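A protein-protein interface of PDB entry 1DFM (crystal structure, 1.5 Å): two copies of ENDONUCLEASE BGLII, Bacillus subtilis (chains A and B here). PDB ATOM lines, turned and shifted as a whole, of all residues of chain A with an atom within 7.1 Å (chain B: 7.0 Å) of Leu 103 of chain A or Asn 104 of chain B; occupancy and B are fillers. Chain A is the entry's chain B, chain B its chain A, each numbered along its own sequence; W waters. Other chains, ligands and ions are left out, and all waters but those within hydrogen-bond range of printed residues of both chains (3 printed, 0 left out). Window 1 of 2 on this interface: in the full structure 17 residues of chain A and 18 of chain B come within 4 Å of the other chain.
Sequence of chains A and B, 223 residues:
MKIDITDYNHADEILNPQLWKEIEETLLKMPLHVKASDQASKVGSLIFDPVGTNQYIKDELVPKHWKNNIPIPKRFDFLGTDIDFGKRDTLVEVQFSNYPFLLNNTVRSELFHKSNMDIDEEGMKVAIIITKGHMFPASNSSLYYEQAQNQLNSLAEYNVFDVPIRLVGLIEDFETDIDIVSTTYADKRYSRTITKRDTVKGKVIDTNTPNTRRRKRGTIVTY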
ATOM      1  N   ASN A  98      12.003 -13.229  28.626  1.00  0.00           N
ATOM      2  CA  ASN A  98      11.142 -14.316  28.259  1.00  0.00           C
ATOM      3  C   ASN A  98      11.157 -14.679  26.794  1.00  0.00           C
ATOM      4  O   ASN A  98      11.472 -13.859  25.927  1.00  0.00           O
ATOM      5  CB  ASN A  98       9.699 -14.206  28.869  1.00  0.00           C
ATOM      6  CG  ASN A  98       8.882 -13.003  28.397  1.00  0.00           C
ATOM      7  OD1 ASN A  98       7.623 -13.133  28.318  1.00  0.00           O
ATOM      8  ND2 ASN A  98       9.504 -11.898  28.137  1.00  0.00           N
ATOM      9  N   TYR A  99      10.876 -15.961  26.577  1.00  0.00           N
ATOM     10  CA  TYR A  99      11.017 -16.554  25.226  1.00  0.00           C
ATOM     11  C   TYR A  99      10.423 -15.799  24.024  1.00  0.00           C
ATOM     12  O   TYR A  99      10.993 -15.891  22.935  1.00  0.00           O
ATOM     13  CB  TYR A  99      10.594 -18.035  25.242  1.00  0.00           C
ATOM     14  CG  TYR A  99       9.133 -18.241  25.470  1.00  0.00           C
ATOM     15  CD1 TYR A  99       8.643 -18.318  26.762  1.00  0.00           C
ATOM     16  CD2 TYR A  99       8.235 -18.299  24.402  1.00  0.00           C
ATOM     17  CE1 TYR A  99       7.276 -18.448  27.005  1.00  0.00           C
ATOM     18  CE2 TYR A  99       6.830 -18.438  24.618  1.00  0.00           C
ATOM     19  CZ  TYR A  99       6.379 -18.509  25.930  1.00  0.00           C
ATOM     20  OH  TYR A  99       5.028 -18.635  26.180  1.00  0.00           O
ATOM     21  N   PRO A 100       9.297 -15.076  24.186  1.00  0.00           N
ATOM     22  CA  PRO A 100       8.828 -14.370  22.958  1.00  0.00           C
ATOM     23  C   PRO A 100       9.800 -13.336  22.482  1.00  0.00           C
ATOM     24  O   PRO A 100       9.724 -12.914  21.315  1.00  0.00           O
ATOM     25  CB  PRO A 100       7.477 -13.740  23.364  1.00  0.00           C
ATOM     26  CG  PRO A 100       7.575 -13.613  24.885  1.00  0.00           C
ATOM     27  CD  PRO A 100       8.336 -14.912  25.307  1.00  0.00           C
ATOM     28  N   PHE A 101      10.720 -12.867  23.332  1.00  0.00           N
ATOM     29  CA  PHE A 101      11.732 -11.924  22.876  1.00  0.00           C
ATOM     30  C   PHE A 101      12.586 -12.481  21.748  1.00  0.00           C
ATOM     31  O   PHE A 101      13.168 -11.699  20.965  1.00  0.00           O
ATOM     32  CB  PHE A 101      12.620 -11.488  24.032  1.00  0.00           C
ATOM     33  CG  PHE A 101      12.094 -10.276  24.750  1.00  0.00           C
ATOM     34  CD1 PHE A 101      12.079  -9.053  24.102  1.00  0.00           C
ATOM     35  CD2 PHE A 101      11.632 -10.362  26.072  1.00  0.00           C
ATOM     36  CE1 PHE A 101      11.620  -7.899  24.763  1.00  0.00           C
ATOM     37  CE2 PHE A 101      11.165  -9.228  26.757  1.00  0.00           C
ATOM     38  CZ  PHE A 101      11.158  -7.977  26.113  1.00  0.00           C
ATOM     39  N   LEU A 102      12.680 -13.808  21.632  1.00  0.00           N
ATOM     40  CA  LEU A 102      13.491 -14.334  20.533  1.00  0.00           C
ATOM     41  C   LEU A 102      12.893 -13.921  19.192  1.00  0.00           C
ATOM     42  O   LEU A 102      13.610 -13.403  18.333  1.00  0.00           O
ATOM     43  CB  LEU A 102      13.640 -15.866  20.648  1.00  0.00           C
ATOM     44  CG  LEU A 102      14.515 -16.596  19.573  1.00  0.00           C
ATOM     45  CD1 LEU A 102      13.748 -16.898  18.341  1.00  0.00           C
ATOM     46  CD2 LEU A 102      15.807 -15.805  19.301  1.00  0.00           C
ATOM     47  N   LEU A 103      11.590 -14.130  19.019  1.00  0.00           N
ATOM     48  CA  LEU A 103      10.950 -13.773  17.751  1.00  0.00           C
ATOM     49  C   LEU A 103      10.799 -12.268  17.603  1.00  0.00           C
ATOM     50  O   LEU A 103      10.870 -11.764  16.471  1.00  0.00           O
ATOM     51  CB  LEU A 103       9.636 -14.543  17.584  1.00  0.00           C
ATOM     52  CG  LEU A 103       9.951 -16.042  17.368  1.00  0.00           C
ATOM     53  CD1 LEU A 103       8.649 -16.843  17.310  1.00  0.00           C
ATOM     54  CD2 LEU A 103      10.711 -16.213  16.048  1.00  0.00           C
ATOM     55  N   ASN A 104      10.630 -11.524  18.701  1.00  0.00           N
ATOM     56  CA  ASN A 104      10.566 -10.064  18.596  1.00  0.00           C
ATOM     57  C   ASN A 104      11.927  -9.552  18.125  1.00  0.00           C
ATOM     58  O   ASN A 104      11.969  -8.721  17.191  1.00  0.00           O
ATOM     59  CB  ASN A 104      10.146  -9.442  19.948  1.00  0.00           C
ATOM     60  CG  ASN A 104      10.508  -7.957  20.071  1.00  0.00           C
ATOM     61  OD1 ASN A 104      11.668  -7.595  20.230  1.00  0.00           O
ATOM     62  ND2 ASN A 104       9.489  -7.082  20.011  1.00  0.00           N
ATOM     63  N   ASN A 105      13.026 -10.071  18.705  1.00  0.00           N
ATOM     64  CA  ASN A 105      14.370  -9.626  18.318  1.00  0.00           C
ATOM     65  C   ASN A 105      14.714 -10.042  16.886  1.00  0.00           C
ATOM     66  O   ASN A 105      15.396  -9.300  16.170  1.00  0.00           O
ATOM     67  CB  ASN A 105      15.423 -10.197  19.266  1.00  0.00           C
ATOM     68  CG  ASN A 105      15.489  -9.488  20.616  1.00  0.00           C
ATOM     69  OD1 ASN A 105      16.389  -9.777  21.401  1.00  0.00           O
ATOM     70  ND2 ASN A 105      14.583  -8.548  20.893  1.00  0.00           N
ATOM     71  N   THR A 106      14.249 -11.214  16.491  1.00  0.00           N
ATOM     72  CA  THR A 106      14.488 -11.697  15.120  1.00  0.00           C
ATOM     73  C   THR A 106      13.737 -10.846  14.109  1.00  0.00           C
ATOM     74  O   THR A 106      14.319 -10.411  13.084  1.00  0.00           O
ATOM     75  CB  THR A 106      14.027 -13.165  15.000  1.00  0.00           C
ATOM     76  OG1 THR A 106      14.847 -13.962  15.868  1.00  0.00           O
ATOM     77  CG2 THR A 106      14.204 -13.691  13.588  1.00  0.00           C
ATOM     78  N   VAL A 107      12.445 -10.608  14.340  1.00  0.00           N
ATOM     79  CA  VAL A 107      11.691  -9.837  13.372  1.00  0.00           C
ATOM     80  C   VAL A 107      12.151  -8.401  13.303  1.00  0.00           C
ATOM     81  O   VAL A 107      12.282  -7.814  12.211  1.00  0.00           O
ATOM     82  CB  VAL A 107      10.177  -9.942  13.671  1.00  0.00           C
ATOM     83  CG1 VAL A 107       9.400  -9.008  12.766  1.00  0.00           C
ATOM     84  CG2 VAL A 107       9.771 -11.379  13.447  1.00  0.00           C
ATOM     85  N   ARG A 108      12.448  -7.780  14.439  1.00  0.00           N
ATOM     86  CA  ARG A 108      12.867  -6.409  14.289  1.00  0.00           C
ATOM     87  C   ARG A 108      14.253  -6.339  13.596  1.00  0.00           C
ATOM     88  O   ARG A 108      14.488  -5.432  12.797  1.00  0.00           O
ATOM     89  CB  ARG A 108      12.726  -5.666  15.609  1.00  0.00           C
ATOM     90  CG  ARG A 108      13.846  -5.925  16.534  1.00  0.00           C
ATOM     91  CD  ARG A 108      13.485  -5.258  17.930  1.00  0.00           C
ATOM     92  NE  ARG A 108      14.712  -4.989  18.667  1.00  0.00           N
ATOM     93  CZ  ARG A 108      14.883  -4.075  19.606  1.00  0.00           C
ATOM     94  NH1 ARG A 108      13.874  -3.283  19.950  1.00  0.00           N
ATOM     95  NH2 ARG A 108      16.071  -3.978  20.213  1.00  0.00           N
ATOM     96  N   SER A 109      15.114  -7.348  13.774  1.00  0.00           N
ATOM     97  CA  SER A 109      16.425  -7.369  13.082  1.00  0.00           C
ATOM     98  C   SER A 109      16.170  -7.517  11.597  1.00  0.00           C
ATOM     99  O   SER A 109      16.877  -6.899  10.808  1.00  0.00           O
ATOM    100  CB  SER A 109      17.308  -8.514  13.579  1.00  0.00           C
ATOM    101  OG  SER A 109      17.637  -8.278  14.940  1.00  0.00           O
ATOM    102  N   LEU A 143      14.290 -17.279  27.917  1.00  0.00           N
ATOM    103  CA  LEU A 143      14.728 -17.916  26.675  1.00  0.00           C
ATOM    104  C   LEU A 143      15.941 -18.813  26.877  1.00  0.00           C
ATOM    105  O   LEU A 143      16.773 -18.530  27.726  1.00  0.00           O
ATOM    106  CB  LEU A 143      15.102 -16.813  25.677  1.00  0.00           C
ATOM    107  CG  LEU A 143      15.626 -17.229  24.291  1.00  0.00           C
ATOM    108  CD1 LEU A 143      14.489 -17.898  23.472  1.00  0.00           C
ATOM    109  CD2 LEU A 143      16.125 -15.988  23.534  1.00  0.00           C
ATOM    110  N   GLN A 147      15.713 -23.749  22.348  1.00  0.00           N
ATOM    111  CA  GLN A 147      14.399 -23.296  21.976  1.00  0.00           C
ATOM    112  C   GLN A 147      14.613 -22.264  20.850  1.00  0.00           C
ATOM    113  O   GLN A 147      13.890 -22.291  19.826  1.00  0.00           O
ATOM    114  CB  GLN A 147      13.775 -22.683  23.225  1.00  0.00           C
ATOM    115  CG  GLN A 147      12.763 -21.628  22.991  1.00  0.00           C
ATOM    116  CD  GLN A 147      12.225 -21.107  24.296  1.00  0.00           C
ATOM    117  OE1 GLN A 147      12.965 -20.557  25.158  1.00  0.00           O
ATOM    118  NE2 GLN A 147      10.923 -21.268  24.446  1.00  0.00           N
ATOM    119  N   ALA A 148      15.592 -21.374  21.021  1.00  0.00           N
ATOM    120  CA  ALA A 148      15.844 -20.388  19.968  1.00  0.00           C
ATOM    121  C   ALA A 148      16.261 -21.085  18.664  1.00  0.00           C
ATOM    122  O   ALA A 148      15.830 -20.716  17.582  1.00  0.00           O
ATOM    123  CB  ALA A 148      16.930 -19.418  20.421  1.00  0.00           C
ATOM    124  N   GLN A 151      13.242 -22.737  17.024  1.00  0.00           N
ATOM    125  CA  GLN A 151      12.377 -21.742  16.380  1.00  0.00           C
ATOM    126  C   GLN A 151      12.997 -21.169  15.126  1.00  0.00           C
ATOM    127  O   GLN A 151      12.332 -21.122  14.080  1.00  0.00           O
ATOM    128  CB  GLN A 151      12.013 -20.627  17.356  1.00  0.00           C
ATOM    129  CG  GLN A 151      11.132 -21.135  18.493  1.00  0.00           C
ATOM    130  CD  GLN A 151      10.488 -20.035  19.312  1.00  0.00           C
ATOM    131  OE1 GLN A 151      10.855 -18.862  19.207  1.00  0.00           O
ATOM    132  NE2 GLN A 151       9.529 -20.415  20.156  1.00  0.00           N
ATOM    133  N   LEU A 152      14.256 -20.746  15.185  1.00  0.00           N
ATOM    134  CA  LEU A 152      14.862 -20.177  13.979  1.00  0.00           C
ATOM    135  C   LEU A 152      15.059 -21.247  12.899  1.00  0.00           C
ATOM    136  O   LEU A 152      14.984 -20.914  11.689  1.00  0.00           O
ATOM    137  CB  LEU A 152      16.208 -19.519  14.317  1.00  0.00           C
ATOM    138  CG  LEU A 152      16.073 -18.271  15.212  1.00  0.00           C
ATOM    139  CD1 LEU A 152      17.475 -17.684  15.478  1.00  0.00           C
ATOM    140  CD2 LEU A 152      15.150 -17.262  14.524  1.00  0.00           C
ATOM    141  N   LEU A 155      11.786 -21.416  11.128  1.00  0.00           N
ATOM    142  CA  LEU A 155      11.629 -20.238  10.258  1.00  0.00           C
ATOM    143  C   LEU A 155      12.508 -20.393   9.014  1.00  0.00           C
ATOM    144  O   LEU A 155      12.072 -20.036   7.906  1.00  0.00           O
ATOM    145  CB  LEU A 155      12.041 -18.950  10.968  1.00  0.00           C
ATOM    146  CG  LEU A 155      10.925 -18.330  11.793  1.00  0.00           C
ATOM    147  CD1 LEU A 155      10.478 -19.258  12.874  1.00  0.00           C
ATOM    148  CD2 LEU A 155      11.455 -17.011  12.396  1.00  0.00           C
ATOM    149  N   PHE B  78       8.017 -26.817  19.573  1.00  0.00           N
ATOM    150  CA  PHE B  78       8.977 -25.775  19.955  1.00  0.00           C
ATOM    151  C   PHE B  78       8.331 -24.387  19.757  1.00  0.00           C
ATOM    152  O   PHE B  78       8.911 -23.388  20.174  1.00  0.00           O
ATOM    153  CB  PHE B  78      10.258 -25.889  19.092  1.00  0.00           C
ATOM    154  CG  PHE B  78       9.978 -26.000  17.636  1.00  0.00           C
ATOM    155  CD1 PHE B  78       9.756 -24.854  16.862  1.00  0.00           C
ATOM    156  CD2 PHE B  78       9.810 -27.245  17.051  1.00  0.00           C
ATOM    157  CE1 PHE B  78       9.361 -24.962  15.549  1.00  0.00           C
ATOM    158  CE2 PHE B  78       9.416 -27.356  15.732  1.00  0.00           C
ATOM    159  CZ  PHE B  78       9.190 -26.205  14.988  1.00  0.00           C
ATOM    160  N   LEU B  79       7.148 -24.327  19.118  1.00  0.00           N
ATOM    161  CA  LEU B  79       6.448 -23.038  18.956  1.00  0.00           C
ATOM    162  C   LEU B  79       5.486 -22.813  20.106  1.00  0.00           C
ATOM    163  O   LEU B  79       4.937 -21.728  20.259  1.00  0.00           O
ATOM    164  CB  LEU B  79       5.662 -22.971  17.640  1.00  0.00           C
ATOM    165  CG  LEU B  79       6.570 -22.898  16.416  1.00  0.00           C
ATOM    166  CD1 LEU B  79       5.664 -22.778  15.203  1.00  0.00           C
ATOM    167  CD2 LEU B  79       7.484 -21.688  16.481  1.00  0.00           C
ATOM    168  N   GLY B  80       5.248 -23.854  20.894  1.00  0.00           N
ATOM    169  CA  GLY B  80       4.379 -23.662  22.044  1.00  0.00           C
ATOM    170  C   GLY B  80       3.567 -24.889  22.359  1.00  0.00           C
ATOM    171  O   GLY B  80       3.619 -25.854  21.586  1.00  0.00           O
ATOM    172  N   GLN B  95      -4.163 -11.331  23.800  1.00  0.00           N
ATOM    173  CA  GLN B  95      -2.803 -11.060  24.212  1.00  0.00           C
ATOM    174  C   GLN B  95      -2.590  -9.764  24.954  1.00  0.00           C
ATOM    175  O   GLN B  95      -2.375  -8.709  24.350  1.00  0.00           O
ATOM    176  CB  GLN B  95      -1.951 -11.130  22.917  1.00  0.00           C
ATOM    177  CG  GLN B  95      -0.422 -11.170  23.158  1.00  0.00           C
ATOM    178  CD  GLN B  95      -0.063 -12.204  24.204  1.00  0.00           C
ATOM    179  OE1 GLN B  95       0.016 -11.870  25.409  1.00  0.00           O
ATOM    180  NE2 GLN B  95       0.117 -13.449  23.787  1.00  0.00           N
ATOM    181  N   TYR B  99       4.816  -7.022  25.309  1.00  0.00           N
ATOM    182  CA  TYR B  99       4.799  -6.777  23.864  1.00  0.00           C
ATOM    183  C   TYR B  99       5.494  -7.774  22.942  1.00  0.00           C
ATOM    184  O   TYR B  99       5.023  -8.000  21.835  1.00  0.00           O
ATOM    185  CB  TYR B  99       5.241  -5.330  23.587  1.00  0.00           C
ATOM    186  CG  TYR B  99       6.674  -5.095  23.922  1.00  0.00           C
ATOM    187  CD1 TYR B  99       7.678  -5.337  23.000  1.00  0.00           C
ATOM    188  CD2 TYR B  99       7.037  -4.673  25.193  1.00  0.00           C
ATOM    189  CE1 TYR B  99       9.046  -5.174  23.349  1.00  0.00           C
ATOM    190  CE2 TYR B  99       8.379  -4.506  25.578  1.00  0.00           C
ATOM    191  CZ  TYR B  99       9.394  -4.757  24.651  1.00  0.00           C
ATOM    192  OH  TYR B  99      10.718  -4.560  24.997  1.00  0.00           O
ATOM    193  N   PRO B 100       6.611  -8.407  23.349  1.00  0.00           N
ATOM    194  CA  PRO B 100       7.157  -9.331  22.359  1.00  0.00           C
ATOM    195  C   PRO B 100       6.242 -10.456  21.985  1.00  0.00           C
ATOM    196  O   PRO B 100       6.396 -11.080  20.913  1.00  0.00           O
ATOM    197  CB  PRO B 100       8.461  -9.832  23.006  1.00  0.00           C
ATOM    198  CG  PRO B 100       8.206  -9.691  24.445  1.00  0.00           C
ATOM    199  CD  PRO B 100       7.457  -8.351  24.561  1.00  0.00           C
ATOM    200  N   PHE B 101       5.228 -10.748  22.836  1.00  0.00           N
ATOM    201  CA  PHE B 101       4.323 -11.847  22.493  1.00  0.00           C
ATOM    202  C   PHE B 101       3.568 -11.569  21.200  1.00  0.00           C
ATOM    203  O   PHE B 101       3.077 -12.499  20.567  1.00  0.00           O
ATOM    204  CB  PHE B 101       3.308 -12.072  23.614  1.00  0.00           C
ATOM    205  CG  PHE B 101       3.718 -13.115  24.610  1.00  0.00           C
ATOM    206  CD1 PHE B 101       3.785 -14.440  24.255  1.00  0.00           C
ATOM    207  CD2 PHE B 101       4.041 -12.739  25.902  1.00  0.00           C
ATOM    208  CE1 PHE B 101       4.190 -15.412  25.204  1.00  0.00           C
ATOM    209  CE2 PHE B 101       4.427 -13.675  26.833  1.00  0.00           C
ATOM    210  CZ  PHE B 101       4.501 -14.987  26.501  1.00  0.00           C
ATOM    211  N   LEU B 102       3.434 -10.298  20.813  1.00  0.00           N
ATOM    212  CA  LEU B 102       2.749 -10.041  19.514  1.00  0.00           C
ATOM    213  C   LEU B 102       3.496 -10.695  18.358  1.00  0.00           C
ATOM    214  O   LEU B 102       2.905 -11.373  17.529  1.00  0.00           O
ATOM    215  CB  LEU B 102       2.647  -8.526  19.260  1.00  0.00           C
ATOM    216  CG  LEU B 102       1.951  -7.944  17.981  1.00  0.00           C
ATOM    217  CD1 LEU B 102       2.828  -7.951  16.765  1.00  0.00           C
ATOM    218  CD2 LEU B 102       0.644  -8.651  17.772  1.00  0.00           C
ATOM    219  N   LEU B 103       4.807 -10.498  18.308  1.00  0.00           N
ATOM    220  CA  LEU B 103       5.576 -11.076  17.199  1.00  0.00           C
ATOM    221  C   LEU B 103       5.734 -12.577  17.349  1.00  0.00           C
ATOM    222  O   LEU B 103       5.781 -13.277  16.355  1.00  0.00           O
ATOM    223  CB  LEU B 103       6.904 -10.333  17.057  1.00  0.00           C
ATOM    224  CG  LEU B 103       6.639  -8.906  16.556  1.00  0.00           C
ATOM    225  CD1 LEU B 103       7.954  -8.146  16.464  1.00  0.00           C
ATOM    226  CD2 LEU B 103       5.935  -8.960  15.207  1.00  0.00           C
ATOM    227  N   ASN B 104       5.836 -13.068  18.585  1.00  0.00           N
ATOM    228  CA  ASN B 104       5.864 -14.492  18.782  1.00  0.00           C
ATOM    229  C   ASN B 104       4.530 -15.102  18.248  1.00  0.00           C
ATOM    230  O   ASN B 104       4.541 -16.124  17.500  1.00  0.00           O
ATOM    231  CB  ASN B 104       6.052 -14.794  20.285  1.00  0.00           C
ATOM    232  CG  ASN B 104       5.724 -16.250  20.630  1.00  0.00           C
ATOM    233  OD1 ASN B 104       4.559 -16.630  20.703  1.00  0.00           O
ATOM    234  ND2 ASN B 104       6.773 -17.076  20.853  1.00  0.00           N
ATOM    235  N   ASN B 105       3.405 -14.476  18.609  1.00  0.00           N
ATOM    236  CA  ASN B 105       2.107 -15.013  18.213  1.00  0.00           C
ATOM    237  C   ASN B 105       1.899 -14.878  16.699  1.00  0.00           C
ATOM    238  O   ASN B 105       1.336 -15.774  16.058  1.00  0.00           O
ATOM    239  CB  ASN B 105       0.959 -14.299  18.960  1.00  0.00           C
ATOM    240  CG  ASN B 105       0.793 -14.727  20.434  1.00  0.00           C
ATOM    241  OD1 ASN B 105      -0.145 -14.239  21.105  1.00  0.00           O
ATOM    242  ND2 ASN B 105       1.655 -15.620  20.933  1.00  0.00           N
ATOM    243  N   THR B 106       2.380 -13.782  16.132  1.00  0.00           N
ATOM    244  CA  THR B 106       2.253 -13.574  14.674  1.00  0.00           C
ATOM    245  C   THR B 106       3.075 -14.587  13.903  1.00  0.00           C
ATOM    246  O   THR B 106       2.592 -15.249  12.994  1.00  0.00           O
ATOM    247  CB  THR B 106       2.694 -12.170  14.320  1.00  0.00           C
ATOM    248  OG1 THR B 106       1.800 -11.242  14.942  1.00  0.00           O
ATOM    249  CG2 THR B 106       2.675 -11.942  12.784  1.00  0.00           C
ATOM    250  N   VAL B 107       4.340 -14.716  14.267  1.00  0.00           N
ATOM    251  CA  VAL B 107       5.184 -15.643  13.564  1.00  0.00           C
ATOM    252  C   VAL B 107       4.725 -17.104  13.730  1.00  0.00           C
ATOM    253  O   VAL B 107       4.679 -17.881  12.745  1.00  0.00           O
ATOM    254  CB  VAL B 107       6.652 -15.443  14.013  1.00  0.00           C
ATOM    255  CG1 VAL B 107       7.538 -16.542  13.430  1.00  0.00           C
ATOM    256  CG2 VAL B 107       7.147 -14.086  13.527  1.00  0.00           C
ATOM    257  N   ARG B 108       4.356 -17.526  14.936  1.00  0.00           N
ATOM    258  CA  ARG B 108       3.946 -18.922  14.991  1.00  0.00           C
ATOM    259  C   ARG B 108       2.655 -19.153  14.196  1.00  0.00           C
ATOM    260  O   ARG B 108       2.518 -20.206  13.600  1.00  0.00           O
ATOM    261  CB  ARG B 108       3.887 -19.437  16.433  1.00  0.00           C
ATOM    262  CG  ARG B 108       2.697 -18.966  17.238  1.00  0.00           C
ATOM    263  CD  ARG B 108       2.874 -19.485  18.688  1.00  0.00           C
ATOM    264  NE  ARG B 108       1.591 -19.438  19.360  1.00  0.00           N
ATOM    265  CZ  ARG B 108       1.321 -20.015  20.520  1.00  0.00           C
ATOM    266  NH1 ARG B 108       2.248 -20.706  21.165  1.00  0.00           N
ATOM    267  NH2 ARG B 108       0.099 -19.875  21.023  1.00  0.00           N
ATOM    268  N   SER B 109       1.750 -18.183  14.147  1.00  0.00           N
ATOM    269  CA  SER B 109       0.517 -18.317  13.361  1.00  0.00           C
ATOM    270  C   SER B 109       0.867 -18.405  11.890  1.00  0.00           C
ATOM    271  O   SER B 109       0.192 -19.090  11.140  1.00  0.00           O
ATOM    272  CB  SER B 109      -0.392 -17.124  13.595  1.00  0.00           C
ATOM    273  OG  SER B 109      -0.857 -17.172  14.939  1.00  0.00           O
ATOM    274  N   GLU B 110       1.907 -17.686  11.480  1.00  0.00           N
ATOM    275  CA  GLU B 110       2.343 -17.766  10.090  1.00  0.00           C
ATOM    276  C   GLU B 110       2.795 -19.188   9.812  1.00  0.00           C
ATOM    277  O   GLU B 110       2.432 -19.756   8.777  1.00  0.00           O
ATOM    278  CB  GLU B 110       3.504 -16.784   9.825  1.00  0.00           C
ATOM    279  CG  GLU B 110       4.182 -16.947   8.441  1.00  0.00           C
ATOM    280  CD  GLU B 110       3.270 -16.541   7.299  1.00  0.00           C
ATOM    281  OE1 GLU B 110       2.062 -16.321   7.531  1.00  0.00           O
ATOM    282  OE2 GLU B 110       3.769 -16.455   6.149  1.00  0.00           O
ATOM    283  N   LEU B 111       3.579 -19.766  10.706  1.00  0.00           N
ATOM    284  CA  LEU B 111       4.067 -21.127  10.483  1.00  0.00           C
ATOM    285  C   LEU B 111       2.895 -22.124  10.517  1.00  0.00           C
ATOM    286  O   LEU B 111       2.845 -23.045   9.699  1.00  0.00           O
ATOM    287  CB  LEU B 111       5.130 -21.508  11.506  1.00  0.00           C
ATOM    288  CG  LEU B 111       6.425 -20.705  11.333  1.00  0.00           C
ATOM    289  CD1 LEU B 111       7.390 -20.906  12.511  1.00  0.00           C
ATOM    290  CD2 LEU B 111       7.062 -21.129  10.016  1.00  0.00           C
HETATM  291  O   HOH W   1       9.772 -16.716  20.650  1.00  0.00           O
HETATM  292  O   HOH W   2       6.777 -19.881  21.352  1.00  0.00           O
HETATM  293  O   HOH W   3       6.571  -7.331  19.569  1.00  0.00           O
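Hydrophobic or aromatic side chains of chain B within 4 Å of the printed part of chain A: Tyr 99, Pro 100, Phe 101, Leu 103, Val 107 and Leu 111.
Among the printed residues, 15 pairs touch across the chains.
Among the printed residues, no Asp or Glu carboxylate lies within 4 Å of a Lys or Arg side-chain nitrogen of the other chain.
The backbone carbonyl oxygen (O) of Phe 78 of chain B lies within hydrogen-bond range of the side-chain amide nitrogen (NE2) of Gln 151 of chain A, at 3.0 Å.
Among the printed residues, merely in contact across the chains: Asn 98 of chain A with Phe 101 of chain B, Tyr 99 of chain A with Phe 101 of chain B, Pro 100 of chain A with Pro 100 of chain B, Pro 100 of chain A with Phe 101 of chain B, Pro 100 of chain A with Asn 104 of chain B, Phe 101 of chain A with Tyr 99 of chain B, Phe 101 of chain A with Pro 100 of chain B, Leu 103 of chain A with Asn 104 of chain B, Asn 104 of chain A with Tyr 99 of chain B, Asn 104 of chain A with Pro 100 of chain B, Asn 104 of chain A with Leu 103 of chain B, Val 107 of chain A with Leu 103 of chain B, Val 107 of chain A with Val 107 of chain B and Leu 155 of chain A with Leu 111 of chain B.
Tyr 99 of chain A touches Phe 101 of chain B, and with the chains exchanged Phe 101 of chain A touches Tyr 99 of chain B.
Pro 100 of chain A touches Phe 101 of chain B, and with the chains exchanged Phe 101 of chain A touches Pro 100 of chain B.
Leu 103 of chain A touches Asn 104 of chain B, and with the chains exchanged Asn 104 of chain A touches Leu 103 of chain B.
Val 107 of chain A touches Leu 103 of chain B, but with the chains exchanged Leu 103 of chain A does not touch Val 107 of chain B (4.05 Å).
Positions printed for both chains: 99, 100, 101, 102, 103, 104, 105, 106, 107, 108 and 109.
Water W1 lies within hydrogen-bond range of O of Tyr 99 of chain A (2.7 Å), OE1 of Gln 151 of chain A (2.8 Å) and ND2 of Asn 104 of chain B (3.0 Å).
Water W3 lies within hydrogen-bond range of O of Tyr 99 of chain B (2.8 Å) and ND2 of Asn 104 of chain A (3.0 Å).
Water W2 lies within hydrogen-bond range of the backbone carbonyl oxygen of Leu 79 of chain B, the side-chain amide nitrogen of Asn 104 of chain B and the side-chain amide nitrogen of Gln 151 of chain A.
Of the printed residues of chain B, Tyr 99 of chain A touches Phe 101.
Of the printed residues of chain A, Pro 100 of chain B touches Pro 100, Phe 101 and Asn 104.
Of the printed residues of chain B, Asn 98 of chain A touches Phe 101.
Of the printed residues of chain A, Leu 103 of chain B touches Asn 104 (3.9 Å) and Val 107 (3.996 Å).
Printed residues of chain A within 4 Å of Val 107 of chain B: Val 107 (3.8 Å).
Thr 106 of chain B touches none of the printed residues of chain A.
The nearest residue of chain B that does not touch Leu 103 of chain A is Val 107 of chain B (4.05 Å).
The nearest printed residue of chain A that does not touch Asn 104 of chain B is Tyr 99 of chain A (4.004 Å).
The nearest printed residue of chain A that does not touch Leu 103 of chain B is Leu 103 of chain A (4.2 Å).
The backbone carbonyl oxygen of Phe 101 of chain A lies close to the side-chain amide nitrogen of Asn 105 of chain A (3.5 Å).
OD1 of Asn 104 of chain A is in hydrogen-bond range of ND2 of Asn 105 of chain A (3.1 Å).
The side-chain amide nitrogen of Asn 105 of chain B lies close to the backbone carbonyl oxygen of Phe 101 of chain B (3.4 Å).
The side-chain amide nitrogen of Asn 105 of chain B sits at hydrogen-bond distance from the side-chain amide oxygen of Asn 104 of chain B (3.1 Å).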
